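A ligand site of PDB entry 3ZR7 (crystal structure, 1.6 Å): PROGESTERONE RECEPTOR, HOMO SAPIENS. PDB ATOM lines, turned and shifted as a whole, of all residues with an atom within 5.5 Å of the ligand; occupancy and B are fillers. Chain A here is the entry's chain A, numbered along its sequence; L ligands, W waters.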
ATOM      1  N   LEU A  42      -6.661  17.551  -0.299  1.00  0.00           N
ATOM      2  CA  LEU A  42      -8.081  17.883  -0.158  1.00  0.00           C
ATOM      3  C   LEU A  42      -8.515  18.898  -1.208  1.00  0.00           C
ATOM      4  O   LEU A  42      -9.624  18.821  -1.713  1.00  0.00           O
ATOM      5  CB  LEU A  42      -8.399  18.399   1.258  1.00  0.00           C
ATOM      6  CG  LEU A  42      -8.156  17.364   2.362  1.00  0.00           C
ATOM      7  CD1 LEU A  42      -8.205  18.034   3.753  1.00  0.00           C
ATOM      8  CD2 LEU A  42      -9.129  16.197   2.278  1.00  0.00           C
ATOM      9  N   THR A  43      -7.649  19.846  -1.541  1.00  0.00           N
ATOM     10  CA  THR A  43      -7.959  20.807  -2.598  1.00  0.00           C
ATOM     11  C   THR A  43      -8.112  20.109  -3.931  1.00  0.00           C
ATOM     12  O   THR A  43      -9.018  20.417  -4.708  1.00  0.00           O
ATOM     13  CB  THR A  43      -6.876  21.907  -2.693  1.00  0.00           C
ATOM     14  OG1 THR A  43      -6.927  22.702  -1.502  1.00  0.00           O
ATOM     15  CG2 THR A  43      -7.090  22.808  -3.905  1.00  0.00           C
ATOM     16  N   LEU A  45      -8.901  16.958  -4.369  1.00  0.00           N
ATOM     17  CA  LEU A  45     -10.127  16.165  -4.309  1.00  0.00           C
ATOM     18  C   LEU A  45     -11.365  17.054  -4.546  1.00  0.00           C
ATOM     19  O   LEU A  45     -12.325  16.629  -5.211  1.00  0.00           O
ATOM     20  CB  LEU A  45     -10.214  15.420  -2.959  1.00  0.00           C
ATOM     21  CG  LEU A  45      -9.281  14.209  -2.825  1.00  0.00           C
ATOM     22  CD1 LEU A  45      -9.067  13.808  -1.362  1.00  0.00           C
ATOM     23  CD2 LEU A  45      -9.842  13.032  -3.654  1.00  0.00           C
ATOM     24  N   ASN A  46     -11.353  18.281  -4.022  1.00  0.00           N
ATOM     25  CA  ASN A  46     -12.440  19.212  -4.283  1.00  0.00           C
ATOM     26  C   ASN A  46     -12.519  19.684  -5.727  1.00  0.00           C
ATOM     27  O   ASN A  46     -13.602  19.814  -6.260  1.00  0.00           O
ATOM     28  CB  ASN A  46     -12.379  20.431  -3.344  1.00  0.00           C
ATOM     29  CG  ASN A  46     -12.895  20.138  -1.945  1.00  0.00           C
ATOM     30  OD1 ASN A  46     -13.556  19.129  -1.714  1.00  0.00           O
ATOM     31  ND2 ASN A  46     -12.618  21.042  -1.011  1.00  0.00           N
ATOM     32  N   LEU A  48     -11.519  17.815  -8.238  1.00  0.00           N
ATOM     33  CA  LEU A  48     -12.053  16.627  -8.907  1.00  0.00           C
ATOM     34  C   LEU A  48     -13.557  16.565  -8.682  1.00  0.00           C
ATOM     35  O   LEU A  48     -14.311  16.252  -9.591  1.00  0.00           O
ATOM     36  CB  LEU A  48     -11.423  15.352  -8.330  1.00  0.00           C
ATOM     37  CG  LEU A  48     -11.951  14.021  -8.851  1.00  0.00           C
ATOM     38  CD1 LEU A  48     -11.720  13.923 -10.381  1.00  0.00           C
ATOM     39  CD2 LEU A  48     -11.304  12.825  -8.141  1.00  0.00           C
ATOM     40  N   GLY A  49     -13.959  16.843  -7.447  1.00  0.00           N
ATOM     41  CA  GLY A  49     -15.372  16.941  -7.075  1.00  0.00           C
ATOM     42  C   GLY A  49     -16.196  17.870  -7.928  1.00  0.00           C
ATOM     43  O   GLY A  49     -17.299  17.503  -8.373  1.00  0.00           O
ATOM     44  N   GLN A  52     -16.597  16.319 -11.313  1.00  0.00           N
ATOM     45  CA  GLN A  52     -17.578  15.238 -11.247  1.00  0.00           C
ATOM     46  C   GLN A  52     -18.990  15.786 -11.090  1.00  0.00           C
ATOM     47  O   GLN A  52     -19.928  15.234 -11.684  1.00  0.00           O
ATOM     48  CB  GLN A  52     -17.243  14.262 -10.122  1.00  0.00           C
ATOM     49  CG  GLN A  52     -16.018  13.433 -10.450  1.00  0.00           C
ATOM     50  CD  GLN A  52     -15.623  12.563  -9.300  1.00  0.00           C
ATOM     51  OE1 GLN A  52     -16.265  12.577  -8.254  1.00  0.00           O
ATOM     52  NE2 GLN A  52     -14.543  11.804  -9.471  1.00  0.00           N
ATOM     53  N   TRP A  82     -25.500  14.337  -4.454  1.00  0.00           N
ATOM     54  CA  TRP A  82     -24.157  14.405  -5.032  1.00  0.00           C
ATOM     55  C   TRP A  82     -23.094  13.616  -4.269  1.00  0.00           C
ATOM     56  O   TRP A  82     -22.282  12.917  -4.894  1.00  0.00           O
ATOM     57  CB  TRP A  82     -23.716  15.853  -5.260  1.00  0.00           C
ATOM     58  CG  TRP A  82     -23.573  16.636  -3.996  1.00  0.00           C
ATOM     59  CD1 TRP A  82     -24.552  17.306  -3.343  1.00  0.00           C
ATOM     60  CD2 TRP A  82     -22.381  16.827  -3.255  1.00  0.00           C
ATOM     61  NE1 TRP A  82     -24.037  17.902  -2.201  1.00  0.00           N
ATOM     62  CE2 TRP A  82     -22.692  17.625  -2.140  1.00  0.00           C
ATOM     63  CE3 TRP A  82     -21.052  16.394  -3.423  1.00  0.00           C
ATOM     64  CZ2 TRP A  82     -21.737  18.000  -1.198  1.00  0.00           C
ATOM     65  CZ3 TRP A  82     -20.110  16.780  -2.500  1.00  0.00           C
ATOM     66  CH2 TRP A  82     -20.457  17.572  -1.395  1.00  0.00           C
ATOM     67  N   MET A  83     -23.068  13.711  -2.933  1.00  0.00           N
ATOM     68  CA  MET A  83     -22.058  12.972  -2.171  1.00  0.00           C
ATOM     69  C   MET A  83     -22.212  11.476  -2.400  1.00  0.00           C
ATOM     70  O   MET A  83     -21.229  10.767  -2.623  1.00  0.00           O
ATOM     71  CB  MET A  83     -22.132  13.304  -0.676  1.00  0.00           C
ATOM     72  CG  MET A  83     -21.150  12.550   0.158  1.00  0.00           C
ATOM     73  SD  MET A  83     -19.486  13.193  -0.046  1.00  0.00           S
ATOM     74  CE  MET A  83     -19.648  14.685   0.946  1.00  0.00           C
ATOM     75  N   MET A  86     -20.934  10.498  -5.829  1.00  0.00           N
ATOM     76  CA  MET A  86     -19.468  10.549  -5.897  1.00  0.00           C
ATOM     77  C   MET A  86     -18.823   9.336  -5.227  1.00  0.00           C
ATOM     78  O   MET A  86     -17.915   8.722  -5.793  1.00  0.00           O
ATOM     79  CB  MET A  86     -18.919  11.846  -5.306  1.00  0.00           C
ATOM     80  CG  MET A  86     -19.144  13.031  -6.212  1.00  0.00           C
ATOM     81  SD  MET A  86     -18.475  14.546  -5.530  1.00  0.00           S
ATOM     82  CE  MET A  86     -19.285  15.691  -6.638  1.00  0.00           C
ATOM     83  N   VAL A  87     -19.259   9.000  -4.023  1.00  0.00           N
ATOM     84  CA  VAL A  87     -18.626   7.887  -3.318  1.00  0.00           C
ATOM     85  C   VAL A  87     -18.987   6.549  -3.966  1.00  0.00           C
ATOM     86  O   VAL A  87     -18.168   5.613  -3.975  1.00  0.00           O
ATOM     87  CB  VAL A  87     -18.947   7.917  -1.797  1.00  0.00           C
ATOM     88  CG1 VAL A  87     -20.397   7.546  -1.513  1.00  0.00           C
ATOM     89  CG2 VAL A  87     -17.981   7.040  -1.051  1.00  0.00           C
ATOM     90  N   LEU A  90     -16.733   6.365  -6.981  1.00  0.00           N
ATOM     91  CA  LEU A  90     -15.387   6.063  -6.470  1.00  0.00           C
ATOM     92  C   LEU A  90     -15.263   4.553  -6.200  1.00  0.00           C
ATOM     93  O   LEU A  90     -14.259   3.917  -6.530  1.00  0.00           O
ATOM     94  CB  LEU A  90     -15.100   6.854  -5.183  1.00  0.00           C
ATOM     95  CG  LEU A  90     -13.851   6.467  -4.397  1.00  0.00           C
ATOM     96  CD1 LEU A  90     -12.567   6.740  -5.178  1.00  0.00           C
ATOM     97  CD2 LEU A  90     -13.834   7.220  -3.064  1.00  0.00           C
ATOM     98  N   ARG A  93     -15.069   2.692  -9.723  1.00  0.00           N
ATOM     99  CA  ARG A  93     -13.765   2.858 -10.374  1.00  0.00           C
ATOM    100  C   ARG A  93     -12.666   2.088  -9.653  1.00  0.00           C
ATOM    101  O   ARG A  93     -11.765   1.507 -10.274  1.00  0.00           O
ATOM    102  CB  ARG A  93     -13.390   4.344 -10.432  1.00  0.00           C
ATOM    103  CG  ARG A  93     -14.299   5.192 -11.305  1.00  0.00           C
ATOM    104  CD  ARG A  93     -13.701   6.583 -11.528  1.00  0.00           C
ATOM    105  NE  ARG A  93     -13.571   7.333 -10.288  1.00  0.00           N
ATOM    106  CZ  ARG A  93     -14.563   8.026  -9.707  1.00  0.00           C
ATOM    107  NH1 ARG A  93     -15.789   8.041 -10.211  1.00  0.00           N
ATOM    108  NH2 ARG A  93     -14.323   8.696  -8.593  1.00  0.00           N
ATOM    109  N   PHE A 105      -9.697   7.629  -7.180  1.00  0.00           N
ATOM    110  CA  PHE A 105     -10.439   8.892  -7.351  1.00  0.00           C
ATOM    111  C   PHE A 105     -10.416   9.315  -8.807  1.00  0.00           C
ATOM    112  O   PHE A 105     -11.418   9.736  -9.350  1.00  0.00           O
ATOM    113  CB  PHE A 105      -9.866   9.987  -6.443  1.00  0.00           C
ATOM    114  CG  PHE A 105     -10.090   9.754  -4.984  1.00  0.00           C
ATOM    115  CD1 PHE A 105     -11.309  10.075  -4.407  1.00  0.00           C
ATOM    116  CD2 PHE A 105      -9.093   9.208  -4.187  1.00  0.00           C
ATOM    117  CE1 PHE A 105     -11.526   9.856  -3.056  1.00  0.00           C
ATOM    118  CE2 PHE A 105      -9.321   8.981  -2.832  1.00  0.00           C
ATOM    119  CZ  PHE A 105     -10.544   9.310  -2.275  1.00  0.00           C
ATOM    120  N   PHE A 121      -6.435  12.048   6.730  1.00  0.00           N
ATOM    121  CA  PHE A 121      -7.808  11.576   6.775  1.00  0.00           C
ATOM    122  C   PHE A 121      -7.872  10.066   6.492  1.00  0.00           C
ATOM    123  O   PHE A 121      -8.731   9.612   5.751  1.00  0.00           O
ATOM    124  CB  PHE A 121      -8.706  12.388   5.809  1.00  0.00           C
ATOM    125  CG  PHE A 121      -8.160  12.532   4.407  1.00  0.00           C
ATOM    126  CD1 PHE A 121      -7.162  13.462   4.114  1.00  0.00           C
ATOM    127  CD2 PHE A 121      -8.675  11.766   3.367  1.00  0.00           C
ATOM    128  CE1 PHE A 121      -6.675  13.611   2.811  1.00  0.00           C
ATOM    129  CE2 PHE A 121      -8.190  11.905   2.066  1.00  0.00           C
ATOM    130  CZ  PHE A 121      -7.190  12.818   1.794  1.00  0.00           C
ATOM    131  N   LEU A 124     -11.301   8.481   7.176  1.00  0.00           N
ATOM    132  CA  LEU A 124     -12.238   8.781   6.108  1.00  0.00           C
ATOM    133  C   LEU A 124     -11.971   7.857   4.924  1.00  0.00           C
ATOM    134  O   LEU A 124     -12.910   7.356   4.324  1.00  0.00           O
ATOM    135  CB  LEU A 124     -12.137  10.243   5.647  1.00  0.00           C
ATOM    136  CG  LEU A 124     -13.302  10.693   4.759  1.00  0.00           C
ATOM    137  CD1 LEU A 124     -14.600  10.700   5.546  1.00  0.00           C
ATOM    138  CD2 LEU A 124     -13.053  12.038   4.104  1.00  0.00           C
ATOM    139  N   MET A 128     -14.551   5.171   3.183  1.00  0.00           N
ATOM    140  CA  MET A 128     -14.865   5.173   1.748  1.00  0.00           C
ATOM    141  C   MET A 128     -14.470   3.862   1.070  1.00  0.00           C
ATOM    142  O   MET A 128     -15.141   3.418   0.142  1.00  0.00           O
ATOM    143  CB  MET A 128     -14.170   6.341   1.043  1.00  0.00           C
ATOM    144  CG  MET A 128     -14.692   7.725   1.446  1.00  0.00           C
ATOM    145  SD  MET A 128     -13.878   9.008   0.489  1.00  0.00           S
ATOM    146  CE  MET A 128     -12.272   9.101   1.201  1.00  0.00           C
ATOM    147  N   LEU A 214     -19.635  11.165   5.712  1.00  0.00           N
ATOM    148  CA  LEU A 214     -18.967  12.006   4.716  1.00  0.00           C
ATOM    149  C   LEU A 214     -19.553  13.421   4.706  1.00  0.00           C
ATOM    150  O   LEU A 214     -18.822  14.377   4.544  1.00  0.00           O
ATOM    151  CB  LEU A 214     -19.051  11.376   3.305  1.00  0.00           C
ATOM    152  CG  LEU A 214     -18.554   9.932   3.154  1.00  0.00           C
ATOM    153  CD1 LEU A 214     -18.612   9.563   1.668  1.00  0.00           C
ATOM    154  CD2 LEU A 214     -17.177   9.696   3.734  1.00  0.00           C
ATOM    155  N   TYR A 217     -18.041  15.346   7.710  1.00  0.00           N
ATOM    156  CA  TYR A 217     -16.669  15.697   7.344  1.00  0.00           C
ATOM    157  C   TYR A 217     -16.653  16.893   6.382  1.00  0.00           C
ATOM    158  O   TYR A 217     -15.887  17.845   6.576  1.00  0.00           O
ATOM    159  CB  TYR A 217     -15.951  14.487   6.693  1.00  0.00           C
ATOM    160  CG  TYR A 217     -14.506  14.790   6.365  1.00  0.00           C
ATOM    161  CD1 TYR A 217     -14.154  15.377   5.157  1.00  0.00           C
ATOM    162  CD2 TYR A 217     -13.503  14.537   7.276  1.00  0.00           C
ATOM    163  CE1 TYR A 217     -12.839  15.686   4.853  1.00  0.00           C
ATOM    164  CE2 TYR A 217     -12.172  14.846   6.989  1.00  0.00           C
ATOM    165  CZ  TYR A 217     -11.855  15.419   5.782  1.00  0.00           C
ATOM    166  OH  TYR A 217     -10.538  15.710   5.500  1.00  0.00           O
ATOM    167  N   CYS A 218     -17.507  16.828   5.370  1.00  0.00           N
ATOM    168  CA  CYS A 218     -17.623  17.888   4.375  1.00  0.00           C
ATOM    169  C   CYS A 218     -17.971  19.225   5.007  1.00  0.00           C
ATOM    170  O   CYS A 218     -17.295  20.219   4.762  1.00  0.00           O
ATOM    171  CB  CYS A 218     -18.678  17.513   3.325  1.00  0.00           C
ATOM    172  SG  CYS A 218     -18.898  18.779   2.076  1.00  0.00           S
ATOM    173  N   THR A 221     -15.163  20.572   7.117  1.00  0.00           N
ATOM    174  CA  THR A 221     -14.077  21.018   6.236  1.00  0.00           C
ATOM    175  C   THR A 221     -14.398  22.363   5.527  1.00  0.00           C
ATOM    176  O   THR A 221     -13.552  23.247   5.425  1.00  0.00           O
ATOM    177  CB  THR A 221     -13.685  19.907   5.246  1.00  0.00           C
ATOM    178  OG1 THR A 221     -13.317  18.735   5.998  1.00  0.00           O
ATOM    179  CG2 THR A 221     -12.504  20.321   4.395  1.00  0.00           C
ATOM    180  N   VAL A 230      -8.067  24.832   2.300  1.00  0.00           N
ATOM    181  CA  VAL A 230      -8.750  23.902   1.405  1.00  0.00           C
ATOM    182  C   VAL A 230      -9.752  24.711   0.571  1.00  0.00           C
ATOM    183  O   VAL A 230     -10.665  25.323   1.118  1.00  0.00           O
ATOM    184  CB  VAL A 230      -9.453  22.780   2.201  1.00  0.00           C
ATOM    185  CG1 VAL A 230     -10.284  21.892   1.269  1.00  0.00           C
ATOM    186  CG2 VAL A 230      -8.423  21.930   2.927  1.00  0.00           C
ATOM    187  N   PHE A 232     -12.820  25.242  -1.904  1.00  0.00           N
ATOM    188  CA  PHE A 232     -14.063  24.667  -2.393  1.00  0.00           C
ATOM    189  C   PHE A 232     -14.493  25.460  -3.619  1.00  0.00           C
ATOM    190  O   PHE A 232     -14.738  26.640  -3.499  1.00  0.00           O
ATOM    191  CB  PHE A 232     -15.153  24.722  -1.323  1.00  0.00           C
ATOM    192  CG  PHE A 232     -14.997  23.685  -0.269  1.00  0.00           C
ATOM    193  CD1 PHE A 232     -14.071  23.849   0.734  1.00  0.00           C
ATOM    194  CD2 PHE A 232     -15.732  22.503  -0.312  1.00  0.00           C
ATOM    195  CE1 PHE A 232     -13.896  22.889   1.713  1.00  0.00           C
ATOM    196  CE2 PHE A 232     -15.568  21.544   0.660  1.00  0.00           C
ATOM    197  CZ  PHE A 232     -14.642  21.742   1.681  1.00  0.00           C
ATOM    198  N   MET A 236     -19.677  23.280  -6.114  1.00  0.00           N
ATOM    199  CA  MET A 236     -19.598  22.509  -4.879  1.00  0.00           C
ATOM    200  C   MET A 236     -20.011  23.378  -3.682  1.00  0.00           C
ATOM    201  O   MET A 236     -20.747  22.919  -2.821  1.00  0.00           O
ATOM    202  CB  MET A 236     -18.186  21.958  -4.651  1.00  0.00           C
ATOM    203  CG  MET A 236     -18.061  21.211  -3.337  1.00  0.00           C
ATOM    204  SD  MET A 236     -16.471  20.406  -3.152  1.00  0.00           S
ATOM    205  CE  MET A 236     -16.529  19.291  -4.551  1.00  0.00           C
ATOM    206  N   ILE A 240     -23.400  22.738  -1.316  1.00  0.00           N
ATOM    207  CA  ILE A 240     -23.182  22.612   0.138  1.00  0.00           C
ATOM    208  C   ILE A 240     -24.018  23.651   0.880  1.00  0.00           C
ATOM    209  O   ILE A 240     -24.794  23.307   1.781  1.00  0.00           O
ATOM    210  CB  ILE A 240     -21.688  22.743   0.491  1.00  0.00           C
ATOM    211  CG1 ILE A 240     -20.900  21.522   0.051  1.00  0.00           C
ATOM    212  CG2 ILE A 240     -21.529  22.989   2.026  1.00  0.00           C
ATOM    213  CD1 ILE A 240     -19.406  21.741   0.031  1.00  0.00           C
HETATM  214 CL1  LIG L   1     -15.727  13.731   1.413  1.00  0.00          CL
HETATM  215  C1  LIG L   1     -14.266  14.488   0.845  1.00  0.00           C
HETATM  216  N1  LIG L   1     -13.212  13.842   0.305  1.00  0.00           N
HETATM  217  C2  LIG L   1     -13.069  12.397   0.084  1.00  0.00           C
HETATM  218  N2  LIG L   1     -12.251  14.784  -0.021  1.00  0.00           N
HETATM  219  C3  LIG L   1     -12.697  15.959   0.310  1.00  0.00           C
HETATM  220  C4  LIG L   1     -11.945  17.246   0.119  1.00  0.00           C
HETATM  221  C5  LIG L   1     -13.980  15.806   0.870  1.00  0.00           C
HETATM  222  S1  LIG L   1     -14.975  17.144   1.437  1.00  0.00           S
HETATM  223  O1  LIG L   1     -14.149  17.976   2.189  1.00  0.00           O
HETATM  224  O2  LIG L   1     -16.234  16.612   1.822  1.00  0.00           O
HETATM  225  N3  LIG L   1     -15.289  17.960   0.021  1.00  0.00           N
HETATM  226  C6  LIG L   1     -16.357  17.534  -0.906  1.00  0.00           C
HETATM  227  C7  LIG L   1     -16.042  16.241  -1.627  1.00  0.00           C
HETATM  228  C8  LIG L   1     -14.833  16.039  -2.307  1.00  0.00           C
HETATM  229  C9  LIG L   1     -14.568  14.845  -2.972  1.00  0.00           C
HETATM  230  C10 LIG L   1     -16.989  15.214  -1.639  1.00  0.00           C
HETATM  231  C11 LIG L   1     -16.739  14.035  -2.292  1.00  0.00           C
HETATM  232  C12 LIG L   1     -15.519  13.814  -2.952  1.00  0.00           C
HETATM  233  C13 LIG L   1     -15.287  12.516  -3.660  1.00  0.00           C
HETATM  234  C14 LIG L   1     -15.535  11.231  -3.220  1.00  0.00           C
HETATM  235  C15 LIG L   1     -16.077  10.839  -1.888  1.00  0.00           C
HETATM  236  O3  LIG L   1     -15.189  10.422  -4.229  1.00  0.00           O
HETATM  237  N4  LIG L   1     -14.773  11.043  -5.207  1.00  0.00           N
HETATM  238  C16 LIG L   1     -14.788  12.333  -4.973  1.00  0.00           C
HETATM  239  C17 LIG L   1     -14.386  13.459  -5.886  1.00  0.00           C
HETATM  240  O   HOH W   1     -16.370  10.144  -7.566  1.00  0.00           O
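The side-chain sulfur (SD) of Met 236 sits close to the side-chain amide oxygen (OD1) of Asn 46, 3.5 Å away. The side-chain amide nitrogen (NE2) of Gln 52 lies close to the guanidinium group (NH2) of Arg 93 (3.2 Å). The side-chain hydroxyl (OG1) of Thr 221 sits at hydrogen-bond distance from the backbone carbonyl oxygen (O) of Tyr 217 (2.8 Å). O of Phe 105 sits at hydrogen-bond distance from NH2 of Arg 93 (3.2 Å).
Leu 42 touches the ligand. Leu 45 touches the ligand (CD1 to N2, 3.6 Å). Leu 48 touches the ligand. Gly 49 touches the ligand. Gln 52 touches the ligand (OE1 to C17, 3.1 Å). Trp 82 touches the ligand (CZ3 to C10, 3.6 Å). SD of Met 83 touches C10 of the ligand, at 3.6 Å. O of Met 86 touches O3 of the ligand (3.6 Å). Leu 90 touches the ligand (CD2 to O3, 3.7 Å). Phe 105 touches the ligand. Met 128 touches the ligand (SD to C2, 3.5 Å). CE1 of Tyr 217 touches O1 of the ligand, 3.7 Å away. Thr 221 touches the ligand (CG2 to O1, 3.6 Å). CE2 of Phe 232 touches N3 of the ligand, at 3.7 Å. SD of Met 236 touches C6 of the ligand, at 3.6 Å. Hydrophobic or aromatic side chains within 4 Å of the ligand: Leu 42, Leu 45, Leu 48, Trp 82, Met 83, Met 86, Leu 90, Phe 105, Met 128, Tyr 217, Phe 232 and Met 236. 17 residues have an atom within 4 Å of the ligand: Leu 42, Leu 45, Asn 46, Leu 48, Gly 49, Gln 52, Trp 82, Met 83, Met 86, Leu 90, Phe 105, Met 128, Tyr 217, Cys 218, Thr 221, Phe 232 and Met 236. Along chain A the residues within 4 Å of the ligand span positions 42 to 236.
The side-chain amide oxygen (OD1) of Asn 46 sits at hydrogen-bond distance from a nitrogen (N3) of the ligand (2.7 Å). The side-chain sulfur of Cys 218 lies close to an oxygen (O2) of the ligand, 3.4 Å away.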
